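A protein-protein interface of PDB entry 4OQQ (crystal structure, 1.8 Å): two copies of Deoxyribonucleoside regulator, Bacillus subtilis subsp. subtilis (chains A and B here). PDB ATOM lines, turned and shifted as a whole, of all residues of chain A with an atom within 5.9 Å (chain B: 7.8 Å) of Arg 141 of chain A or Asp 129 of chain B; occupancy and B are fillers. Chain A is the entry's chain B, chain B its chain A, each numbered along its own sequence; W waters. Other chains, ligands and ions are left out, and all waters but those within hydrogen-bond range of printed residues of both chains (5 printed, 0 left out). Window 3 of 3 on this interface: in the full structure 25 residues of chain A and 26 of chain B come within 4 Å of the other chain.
NH2 of Arg 141 of chain A is in salt-bridge range of OD1 of Asp 129 of chain B, at 3.2 Å.
The side-chain carboxylate of Asp 140 of chain A is in hydrogen-bond range of the backbone NH of Asp 129 of chain B (2.8 Å).
A ring nitrogen (ND1) of His 142 of chain A sits at hydrogen-bond distance from the guanidinium group (NH1) of Arg 145 of chain A (3.2 Å).
The side-chain carboxylate (OD1) of Asp 140 of chain A sits at hydrogen-bond distance from the backbone NH (N) of His 142 of chain A (2.9 Å).
The backbone carbonyl oxygen of Phe 128 of chain B lies within hydrogen-bond range of the guanidinium group of Arg 210 of chain B (3.0 Å).
O of Tyr 174 of chain B lies within hydrogen-bond range of NH2 of Arg 210 of chain B, 3.1 Å away.
The side-chain carboxylate (OD1) of Asp 140 of chain A is in hydrogen-bond range of the backbone NH (N) of Ile 143 of chain A, 3.0 Å away.
Among the printed residues, merely in contact across the chains: His 142 of chain A with Gly 173 of chain B, Asp 140 of chain A with Phe 128 of chain B and His 142 of chain A with Tyr 174 of chain B.
Arg 141 of chain A touches just one residue of chain B: Asp 129.
Of chain A, only Asp 140 and Arg 141 come within 4 Å of Asp 129 of chain B.
Of chain B, only Phe 128 (3.4 Å) and Asp 129 (2.8 Å) come within 4 Å of Asp 140 of chain A.
Printed residues of chain B within 4 Å of His 142 of chain A: Gly 173 (3.2 Å) and Tyr 174 (3.6 Å).
Printed residues of chain A within 4 Å of Phe 128 of chain B: Asp 140.
The nearest printed residue of chain B that does not touch His 142 of chain A is Asp 129 of chain B (4.2 Å).
Of the 8 printed residues of chain A, 3 touch a printed residue of chain B.
Hydrophobic or aromatic side chains of chain A that line the printed part of chain B: His 142.
Among the printed residues, Asp or Glu carboxylates within 4 Å of a Lys or Arg side-chain nitrogen of the other chain: Arg 141 of chain A with Asp 129 of chain B (3.2 Å).
No position is printed for both chains.
Of the 5 pairs that touch across the chains among the printed residues, none has its exchanged pair printed and touching as well.
Water W2 lies within hydrogen-bond range of the backbone carbonyl oxygen (O) of Gly 173 of chain B and the guanidinium group (NH1) of Arg 141 of chain A.
Water W3 lies within hydrogen-bond range of NE2 of His 142 of chain A (2.7 Å), O of Tyr 174 of chain B (2.8 Å), NH1 of Arg 210 of chain B (3.0 Å), OD1 of Asp 129 of chain B (3.1 Å) and NH2 of Arg 141 of chain A (3.3 Å).
Water W4 lies within hydrogen-bond range of the side-chain carboxylate of Asp 140 of chain A (2.7 Å), the backbone NH of Asn 130 of chain B (3.0 Å) and the backbone NH of Asp 129 of chain B (3.3 Å).
Water W5 lies within hydrogen-bond range of the side-chain carboxylate of Asp 129 of chain B and the backbone NH of Arg 141 of chain A.
Water W1 lies within hydrogen-bond range of O of Val 127 of chain B and OD1 of Asp 140 of chain A.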
ATOM      1  N   VAL A 137      12.636  -6.718 -22.993  1.00  0.00           N
ATOM      2  CA  VAL A 137      13.070  -5.436 -23.562  1.00  0.00           C
ATOM      3  C   VAL A 137      12.041  -4.353 -23.318  1.00  0.00           C
ATOM      4  O   VAL A 137      12.384  -3.295 -22.853  1.00  0.00           O
ATOM      5  CB  VAL A 137      13.380  -5.592 -25.058  1.00  0.00           C
ATOM      6  CG1 VAL A 137      13.563  -4.232 -25.746  1.00  0.00           C
ATOM      7  CG2 VAL A 137      14.630  -6.398 -25.175  1.00  0.00           C
ATOM      8  N   LYS A 139       9.982  -4.156 -20.894  1.00  0.00           N
ATOM      9  CA  LYS A 139       9.971  -3.836 -19.486  1.00  0.00           C
ATOM     10  C   LYS A 139      11.238  -3.156 -18.990  1.00  0.00           C
ATOM     11  O   LYS A 139      11.293  -2.728 -17.883  1.00  0.00           O
ATOM     12  CB  LYS A 139       9.729  -5.104 -18.658  1.00  0.00           C
ATOM     13  CG  LYS A 139       8.279  -5.590 -18.730  1.00  0.00           C
ATOM     14  CD  LYS A 139       8.127  -6.968 -18.089  1.00  0.00           C
ATOM     15  CE  LYS A 139       6.875  -7.676 -18.597  1.00  0.00           C
ATOM     16  NZ  LYS A 139       5.652  -6.905 -18.220  1.00  0.00           N
ATOM     17  N   ASP A 140      12.266  -3.039 -19.814  1.00  0.00           N
ATOM     18  CA  ASP A 140      13.458  -2.261 -19.430  1.00  0.00           C
ATOM     19  C   ASP A 140      12.980  -0.861 -19.011  1.00  0.00           C
ATOM     20  O   ASP A 140      12.173  -0.239 -19.668  1.00  0.00           O
ATOM     21  CB  ASP A 140      14.493  -2.207 -20.588  1.00  0.00           C
ATOM     22  CG  ASP A 140      15.609  -1.219 -20.351  1.00  0.00           C
ATOM     23  OD1 ASP A 140      15.446   0.013 -20.635  1.00  0.00           O
ATOM     24  OD2 ASP A 140      16.661  -1.629 -19.845  1.00  0.00           O
ATOM     25  N   ARG A 141      13.525  -0.379 -17.909  1.00  0.00           N
ATOM     26  CA  ARG A 141      13.064   0.844 -17.286  1.00  0.00           C
ATOM     27  C   ARG A 141      13.053   2.019 -18.261  1.00  0.00           C
ATOM     28  O   ARG A 141      12.111   2.817 -18.270  1.00  0.00           O
ATOM     29  CB  ARG A 141      13.972   1.135 -16.080  1.00  0.00           C
ATOM     30  CG  ARG A 141      13.539   2.260 -15.214  1.00  0.00           C
ATOM     31  CD  ARG A 141      14.174   2.137 -13.822  1.00  0.00           C
ATOM     32  NE  ARG A 141      15.638   2.173 -13.851  1.00  0.00           N
ATOM     33  CZ  ARG A 141      16.355   3.293 -13.933  1.00  0.00           C
ATOM     34  NH1 ARG A 141      15.756   4.474 -14.042  1.00  0.00           N
ATOM     35  NH2 ARG A 141      17.671   3.240 -13.924  1.00  0.00           N
ATOM     36  N   HIS A 142      14.083   2.092 -19.086  1.00  0.00           N
ATOM     37  CA  HIS A 142      14.240   3.181 -20.019  1.00  0.00           C
ATOM     38  C   HIS A 142      13.313   2.998 -21.216  1.00  0.00           C
ATOM     39  O   HIS A 142      12.605   3.924 -21.633  1.00  0.00           O
ATOM     40  CB  HIS A 142      15.717   3.333 -20.410  1.00  0.00           C
ATOM     41  CG  HIS A 142      16.654   3.389 -19.236  1.00  0.00           C
ATOM     42  ND1 HIS A 142      16.697   4.446 -18.355  1.00  0.00           N
ATOM     43  CD2 HIS A 142      17.540   2.479 -18.776  1.00  0.00           C
ATOM     44  CE1 HIS A 142      17.601   4.202 -17.425  1.00  0.00           C
ATOM     45  NE2 HIS A 142      18.139   3.016 -17.667  1.00  0.00           N
ATOM     46  N   ILE A 143      13.290   1.805 -21.770  1.00  0.00           N
ATOM     47  CA  ILE A 143      12.381   1.519 -22.884  1.00  0.00           C
ATOM     48  C   ILE A 143      10.912   1.720 -22.528  1.00  0.00           C
ATOM     49  O   ILE A 143      10.146   2.243 -23.312  1.00  0.00           O
ATOM     50  CB  ILE A 143      12.590   0.092 -23.448  1.00  0.00           C
ATOM     51  CG1 ILE A 143      14.011  -0.089 -23.961  1.00  0.00           C
ATOM     52  CG2 ILE A 143      11.500  -0.267 -24.469  1.00  0.00           C
ATOM     53  CD1 ILE A 143      14.436   0.748 -25.173  1.00  0.00           C
ATOM     54  N   GLU A 144      10.531   1.336 -21.331  1.00  0.00           N
ATOM     55  CA  GLU A 144       9.177   1.411 -20.890  1.00  0.00           C
ATOM     56  C   GLU A 144       8.683   2.852 -20.944  1.00  0.00           C
ATOM     57  O   GLU A 144       7.501   3.110 -21.263  1.00  0.00           O
ATOM     58  CB  GLU A 144       9.086   0.829 -19.466  1.00  0.00           C
ATOM     59  CG  GLU A 144       7.676   0.758 -18.868  1.00  0.00           C
ATOM     60  CD  GLU A 144       7.106   2.093 -18.369  1.00  0.00           C
ATOM     61  OE1 GLU A 144       7.877   2.975 -17.923  1.00  0.00           O
ATOM     62  OE2 GLU A 144       5.851   2.265 -18.361  1.00  0.00           O
ATOM     63  N   ARG A 145       9.566   3.801 -20.617  1.00  0.00           N
ATOM     64  CA  ARG A 145       9.178   5.211 -20.686  1.00  0.00           C
ATOM     65  C   ARG A 145       8.838   5.654 -22.115  1.00  0.00           C
ATOM     66  O   ARG A 145       7.916   6.460 -22.319  1.00  0.00           O
ATOM     67  CB  ARG A 145      10.245   6.128 -20.147  1.00  0.00           C
ATOM     68  CG  ARG A 145      10.486   5.999 -18.681  1.00  0.00           C
ATOM     69  CD  ARG A 145      11.482   7.089 -18.286  1.00  0.00           C
ATOM     70  NE  ARG A 145      11.990   6.866 -16.937  1.00  0.00           N
ATOM     71  CZ  ARG A 145      13.198   6.383 -16.625  1.00  0.00           C
ATOM     72  NH1 ARG A 145      14.092   6.047 -17.569  1.00  0.00           N
ATOM     73  NH2 ARG A 145      13.511   6.235 -15.341  1.00  0.00           N
ATOM     74  N   PRO B 125      19.483   0.483 -27.751  1.00  0.00           N
ATOM     75  CA  PRO B 125      19.923   1.560 -26.875  1.00  0.00           C
ATOM     76  C   PRO B 125      21.349   1.328 -26.452  1.00  0.00           C
ATOM     77  O   PRO B 125      21.844   0.219 -26.473  1.00  0.00           O
ATOM     78  CB  PRO B 125      18.961   1.440 -25.680  1.00  0.00           C
ATOM     79  CG  PRO B 125      18.654  -0.018 -25.629  1.00  0.00           C
ATOM     80  CD  PRO B 125      18.569  -0.443 -27.063  1.00  0.00           C
ATOM     81  N   VAL B 127      22.497   1.504 -23.389  1.00  0.00           N
ATOM     82  CA  VAL B 127      22.505   0.854 -22.089  1.00  0.00           C
ATOM     83  C   VAL B 127      21.146   0.264 -21.803  1.00  0.00           C
ATOM     84  O   VAL B 127      20.099   0.860 -22.122  1.00  0.00           O
ATOM     85  CB  VAL B 127      22.883   1.883 -20.986  1.00  0.00           C
ATOM     86  CG1 VAL B 127      22.685   1.321 -19.607  1.00  0.00           C
ATOM     87  CG2 VAL B 127      24.311   2.359 -21.150  1.00  0.00           C
ATOM     88  N   PHE B 128      21.174  -0.939 -21.237  1.00  0.00           N
ATOM     89  CA  PHE B 128      20.038  -1.581 -20.598  1.00  0.00           C
ATOM     90  C   PHE B 128      20.192  -1.508 -19.089  1.00  0.00           C
ATOM     91  O   PHE B 128      21.307  -1.559 -18.543  1.00  0.00           O
ATOM     92  CB  PHE B 128      19.916  -3.076 -21.003  1.00  0.00           C
ATOM     93  CG  PHE B 128      19.361  -3.270 -22.368  1.00  0.00           C
ATOM     94  CD1 PHE B 128      17.993  -3.193 -22.580  1.00  0.00           C
ATOM     95  CD2 PHE B 128      20.200  -3.382 -23.483  1.00  0.00           C
ATOM     96  CE1 PHE B 128      17.456  -3.330 -23.860  1.00  0.00           C
ATOM     97  CE2 PHE B 128      19.652  -3.583 -24.744  1.00  0.00           C
ATOM     98  CZ  PHE B 128      18.306  -3.464 -24.945  1.00  0.00           C
ATOM     99  N   ASP B 129      19.042  -1.417 -18.421  1.00  0.00           N
ATOM    100  CA  ASP B 129      18.990  -1.306 -16.975  1.00  0.00           C
ATOM    101  C   ASP B 129      19.595  -2.532 -16.325  1.00  0.00           C
ATOM    102  O   ASP B 129      20.178  -2.428 -15.258  1.00  0.00           O
ATOM    103  CB  ASP B 129      17.558  -1.106 -16.535  1.00  0.00           C
ATOM    104  CG  ASP B 129      17.433  -0.713 -15.056  1.00  0.00           C
ATOM    105  OD1 ASP B 129      18.151   0.181 -14.557  1.00  0.00           O
ATOM    106  OD2 ASP B 129      16.548  -1.286 -14.419  1.00  0.00           O
ATOM    107  N   ASN B 130      19.520  -3.671 -16.995  1.00  0.00           N
ATOM    108  CA  ASN B 130      19.882  -4.970 -16.428  1.00  0.00           C
ATOM    109  C   ASN B 130      20.765  -5.774 -17.374  1.00  0.00           C
ATOM    110  O   ASN B 130      20.454  -5.916 -18.570  1.00  0.00           O
ATOM    111  CB  ASN B 130      18.651  -5.795 -16.134  1.00  0.00           C
ATOM    112  CG  ASN B 130      19.026  -7.181 -15.724  1.00  0.00           C
ATOM    113  OD1 ASN B 130      18.933  -8.123 -16.499  1.00  0.00           O
ATOM    114  ND2 ASN B 130      19.564  -7.291 -14.554  1.00  0.00           N
ATOM    115  N   ALA B 131      21.893  -6.276 -16.855  1.00  0.00           N
ATOM    116  CA  ALA B 131      22.830  -6.978 -17.717  1.00  0.00           C
ATOM    117  C   ALA B 131      22.239  -8.262 -18.301  1.00  0.00           C
ATOM    118  O   ALA B 131      22.684  -8.682 -19.362  1.00  0.00           O
ATOM    119  CB  ALA B 131      24.115  -7.313 -16.965  1.00  0.00           C
ATOM    120  N   ASP B 132      21.329  -8.928 -17.583  1.00  0.00           N
ATOM    121  CA  ASP B 132      20.713 -10.198 -18.089  1.00  0.00           C
ATOM    122  C   ASP B 132      19.900  -9.902 -19.366  1.00  0.00           C
ATOM    123  O   ASP B 132      19.997 -10.649 -20.333  1.00  0.00           O
ATOM    124  CB  ASP B 132      19.845 -10.920 -17.031  1.00  0.00           C
ATOM    125  CG  ASP B 132      20.661 -11.468 -15.855  1.00  0.00           C
ATOM    126  OD1 ASP B 132      21.845 -11.823 -16.036  1.00  0.00           O
ATOM    127  OD2 ASP B 132      20.118 -11.553 -14.739  1.00  0.00           O
ATOM    128  N   VAL B 133      19.205  -8.760 -19.397  1.00  0.00           N
ATOM    129  CA  VAL B 133      18.456  -8.308 -20.590  1.00  0.00           C
ATOM    130  C   VAL B 133      19.447  -7.964 -21.716  1.00  0.00           C
ATOM    131  O   VAL B 133      19.253  -8.364 -22.864  1.00  0.00           O
ATOM    132  CB  VAL B 133      17.510  -7.105 -20.274  1.00  0.00           C
ATOM    133  CG1 VAL B 133      16.813  -6.616 -21.527  1.00  0.00           C
ATOM    134  CG2 VAL B 133      16.472  -7.489 -19.215  1.00  0.00           C
ATOM    135  N   LYS B 134      20.493  -7.178 -21.410  1.00  0.00           N
ATOM    136  CA  LYS B 134      21.504  -6.862 -22.403  1.00  0.00           C
ATOM    137  C   LYS B 134      22.034  -8.163 -23.046  1.00  0.00           C
ATOM    138  O   LYS B 134      22.191  -8.269 -24.281  1.00  0.00           O
ATOM    139  CB  LYS B 134      22.639  -6.039 -21.745  1.00  0.00           C
ATOM    140  CG  LYS B 134      23.833  -5.820 -22.654  1.00  0.00           C
ATOM    141  CD  LYS B 134      24.878  -6.885 -22.685  1.00  0.00           C
ATOM    142  CE  LYS B 134      26.219  -6.303 -23.124  1.00  0.00           C
ATOM    143  NZ  LYS B 134      27.280  -7.330 -23.135  1.00  0.00           N
ATOM    144  N   LEU B 172      21.614  11.172 -19.257  1.00  0.00           N
ATOM    145  CA  LEU B 172      20.526  10.474 -19.908  1.00  0.00           C
ATOM    146  C   LEU B 172      19.759   9.503 -19.005  1.00  0.00           C
ATOM    147  O   LEU B 172      18.952   8.690 -19.484  1.00  0.00           O
ATOM    148  CB  LEU B 172      21.095   9.744 -21.107  1.00  0.00           C
ATOM    149  CG  LEU B 172      21.479  10.648 -22.274  1.00  0.00           C
ATOM    150  CD1 LEU B 172      22.121   9.832 -23.381  1.00  0.00           C
ATOM    151  CD2 LEU B 172      20.244  11.347 -22.798  1.00  0.00           C
ATOM    152  N   GLY B 173      20.006   9.585 -17.700  1.00  0.00           N
ATOM    153  CA  GLY B 173      19.344   8.707 -16.740  1.00  0.00           C
ATOM    154  C   GLY B 173      19.836   7.276 -16.657  1.00  0.00           C
ATOM    155  O   GLY B 173      19.309   6.487 -15.876  1.00  0.00           O
ATOM    156  N   TYR B 174      20.828   6.910 -17.450  1.00  0.00           N
ATOM    157  CA  TYR B 174      21.306   5.561 -17.407  1.00  0.00           C
ATOM    158  C   TYR B 174      22.030   5.184 -16.111  1.00  0.00           C
ATOM    159  O   TYR B 174      22.097   3.996 -15.785  1.00  0.00           O
ATOM    160  CB  TYR B 174      22.187   5.277 -18.618  1.00  0.00           C
ATOM    161  CG  TYR B 174      21.459   5.256 -19.938  1.00  0.00           C
ATOM    162  CD1 TYR B 174      20.374   4.419 -20.120  1.00  0.00           C
ATOM    163  CD2 TYR B 174      21.874   6.034 -21.020  1.00  0.00           C
ATOM    164  CE1 TYR B 174      19.714   4.350 -21.338  1.00  0.00           C
ATOM    165  CE2 TYR B 174      21.202   6.017 -22.232  1.00  0.00           C
ATOM    166  CZ  TYR B 174      20.121   5.168 -22.394  1.00  0.00           C
ATOM    167  OH  TYR B 174      19.448   5.018 -23.593  1.00  0.00           O
ATOM    168  N   PHE B 175      22.523   6.169 -15.345  1.00  0.00           N
ATOM    169  CA  PHE B 175      23.373   5.876 -14.178  1.00  0.00           C
ATOM    170  C   PHE B 175      22.915   6.553 -12.889  1.00  0.00           C
ATOM    171  O   PHE B 175      22.488   7.701 -12.896  1.00  0.00           O
ATOM    172  CB  PHE B 175      24.814   6.266 -14.482  1.00  0.00           C
ATOM    173  CG  PHE B 175      25.379   5.687 -15.759  1.00  0.00           C
ATOM    174  CD1 PHE B 175      25.374   4.331 -16.000  1.00  0.00           C
ATOM    175  CD2 PHE B 175      25.995   6.503 -16.683  1.00  0.00           C
ATOM    176  CE1 PHE B 175      25.896   3.835 -17.168  1.00  0.00           C
ATOM    177  CE2 PHE B 175      26.525   6.022 -17.833  1.00  0.00           C
ATOM    178  CZ  PHE B 175      26.485   4.665 -18.092  1.00  0.00           C
ATOM    179  N   ASN B 176      22.966   5.836 -11.774  1.00  0.00           N
ATOM    180  CA  ASN B 176      22.514   6.397 -10.502  1.00  0.00           C
ATOM    181  C   ASN B 176      23.659   7.225  -9.907  1.00  0.00           C
ATOM    182  O   ASN B 176      24.697   7.399 -10.551  1.00  0.00           O
ATOM    183  CB  ASN B 176      22.025   5.303  -9.545  1.00  0.00           C
ATOM    184  CG  ASN B 176      23.086   4.232  -9.274  1.00  0.00           C
ATOM    185  OD1 ASN B 176      24.279   4.525  -9.115  1.00  0.00           O
ATOM    186  ND2 ASN B 176      22.647   2.983  -9.216  1.00  0.00           N
ATOM    187  N   GLU B 179      27.045   5.338  -9.639  1.00  0.00           N
ATOM    188  CA  GLU B 179      27.670   5.012 -10.921  1.00  0.00           C
ATOM    189  C   GLU B 179      28.291   6.231 -11.566  1.00  0.00           C
ATOM    190  O   GLU B 179      29.417   6.175 -12.015  1.00  0.00           O
ATOM    191  CB  GLU B 179      26.645   4.378 -11.875  1.00  0.00           C
ATOM    192  CG  GLU B 179      26.153   3.019 -11.381  1.00  0.00           C
ATOM    193  CD  GLU B 179      24.951   2.486 -12.164  1.00  0.00           C
ATOM    194  OE1 GLU B 179      24.004   3.266 -12.428  1.00  0.00           O
ATOM    195  OE2 GLU B 179      24.929   1.273 -12.443  1.00  0.00           O
ATOM    196  N   ALA B 206      30.528  -3.980 -14.121  1.00  0.00           N
ATOM    197  CA  ALA B 206      29.080  -3.966 -13.904  1.00  0.00           C
ATOM    198  C   ALA B 206      28.359  -3.058 -14.912  1.00  0.00           C
ATOM    199  O   ALA B 206      27.390  -3.469 -15.550  1.00  0.00           O
ATOM    200  CB  ALA B 206      28.720  -3.516 -12.496  1.00  0.00           C
ATOM    201  N   ARG B 210      26.303  -4.092 -19.024  1.00  0.00           N
ATOM    202  CA  ARG B 210      24.965  -3.740 -19.473  1.00  0.00           C
ATOM    203  C   ARG B 210      24.937  -2.662 -20.578  1.00  0.00           C
ATOM    204  O   ARG B 210      23.889  -2.176 -20.944  1.00  0.00           O
ATOM    205  CB  ARG B 210      24.067  -3.381 -18.320  1.00  0.00           C
ATOM    206  CG  ARG B 210      24.383  -2.110 -17.548  1.00  0.00           C
ATOM    207  CD  ARG B 210      23.683  -2.107 -16.201  1.00  0.00           C
ATOM    208  NE  ARG B 210      23.886  -0.861 -15.462  1.00  0.00           N
ATOM    209  CZ  ARG B 210      23.269   0.301 -15.699  1.00  0.00           C
ATOM    210  NH1 ARG B 210      22.403   0.453 -16.671  1.00  0.00           N
ATOM    211  NH2 ARG B 210      23.541   1.346 -14.947  1.00  0.00           N
ATOM    212  N   THR B 211      26.102  -2.356 -21.111  1.00  0.00           N
ATOM    213  CA  THR B 211      26.270  -1.421 -22.228  1.00  0.00           C
ATOM    214  C   THR B 211      26.438  -2.171 -23.534  1.00  0.00           C
ATOM    215  O   THR B 211      27.150  -3.205 -23.609  1.00  0.00           O
ATOM    216  CB  THR B 211      27.521  -0.596 -21.973  1.00  0.00           C
ATOM    217  OG1 THR B 211      27.376   0.083 -20.737  1.00  0.00           O
ATOM    218  CG2 THR B 211      27.799   0.377 -23.077  1.00  0.00           C
HETATM  219  O   HOH W   1      17.398   1.086 -22.539  1.00  0.00           O
HETATM  220  O   HOH W   2      17.106   6.991 -14.831  1.00  0.00           O
HETATM  221  O   HOH W   3      20.001   2.192 -15.966  1.00  0.00           O
HETATM  222  O   HOH W   4      17.099  -4.084 -18.772  1.00  0.00           O
HETATM  223  O   HOH W   5      14.484  -2.268 -15.888  1.00  0.00           O
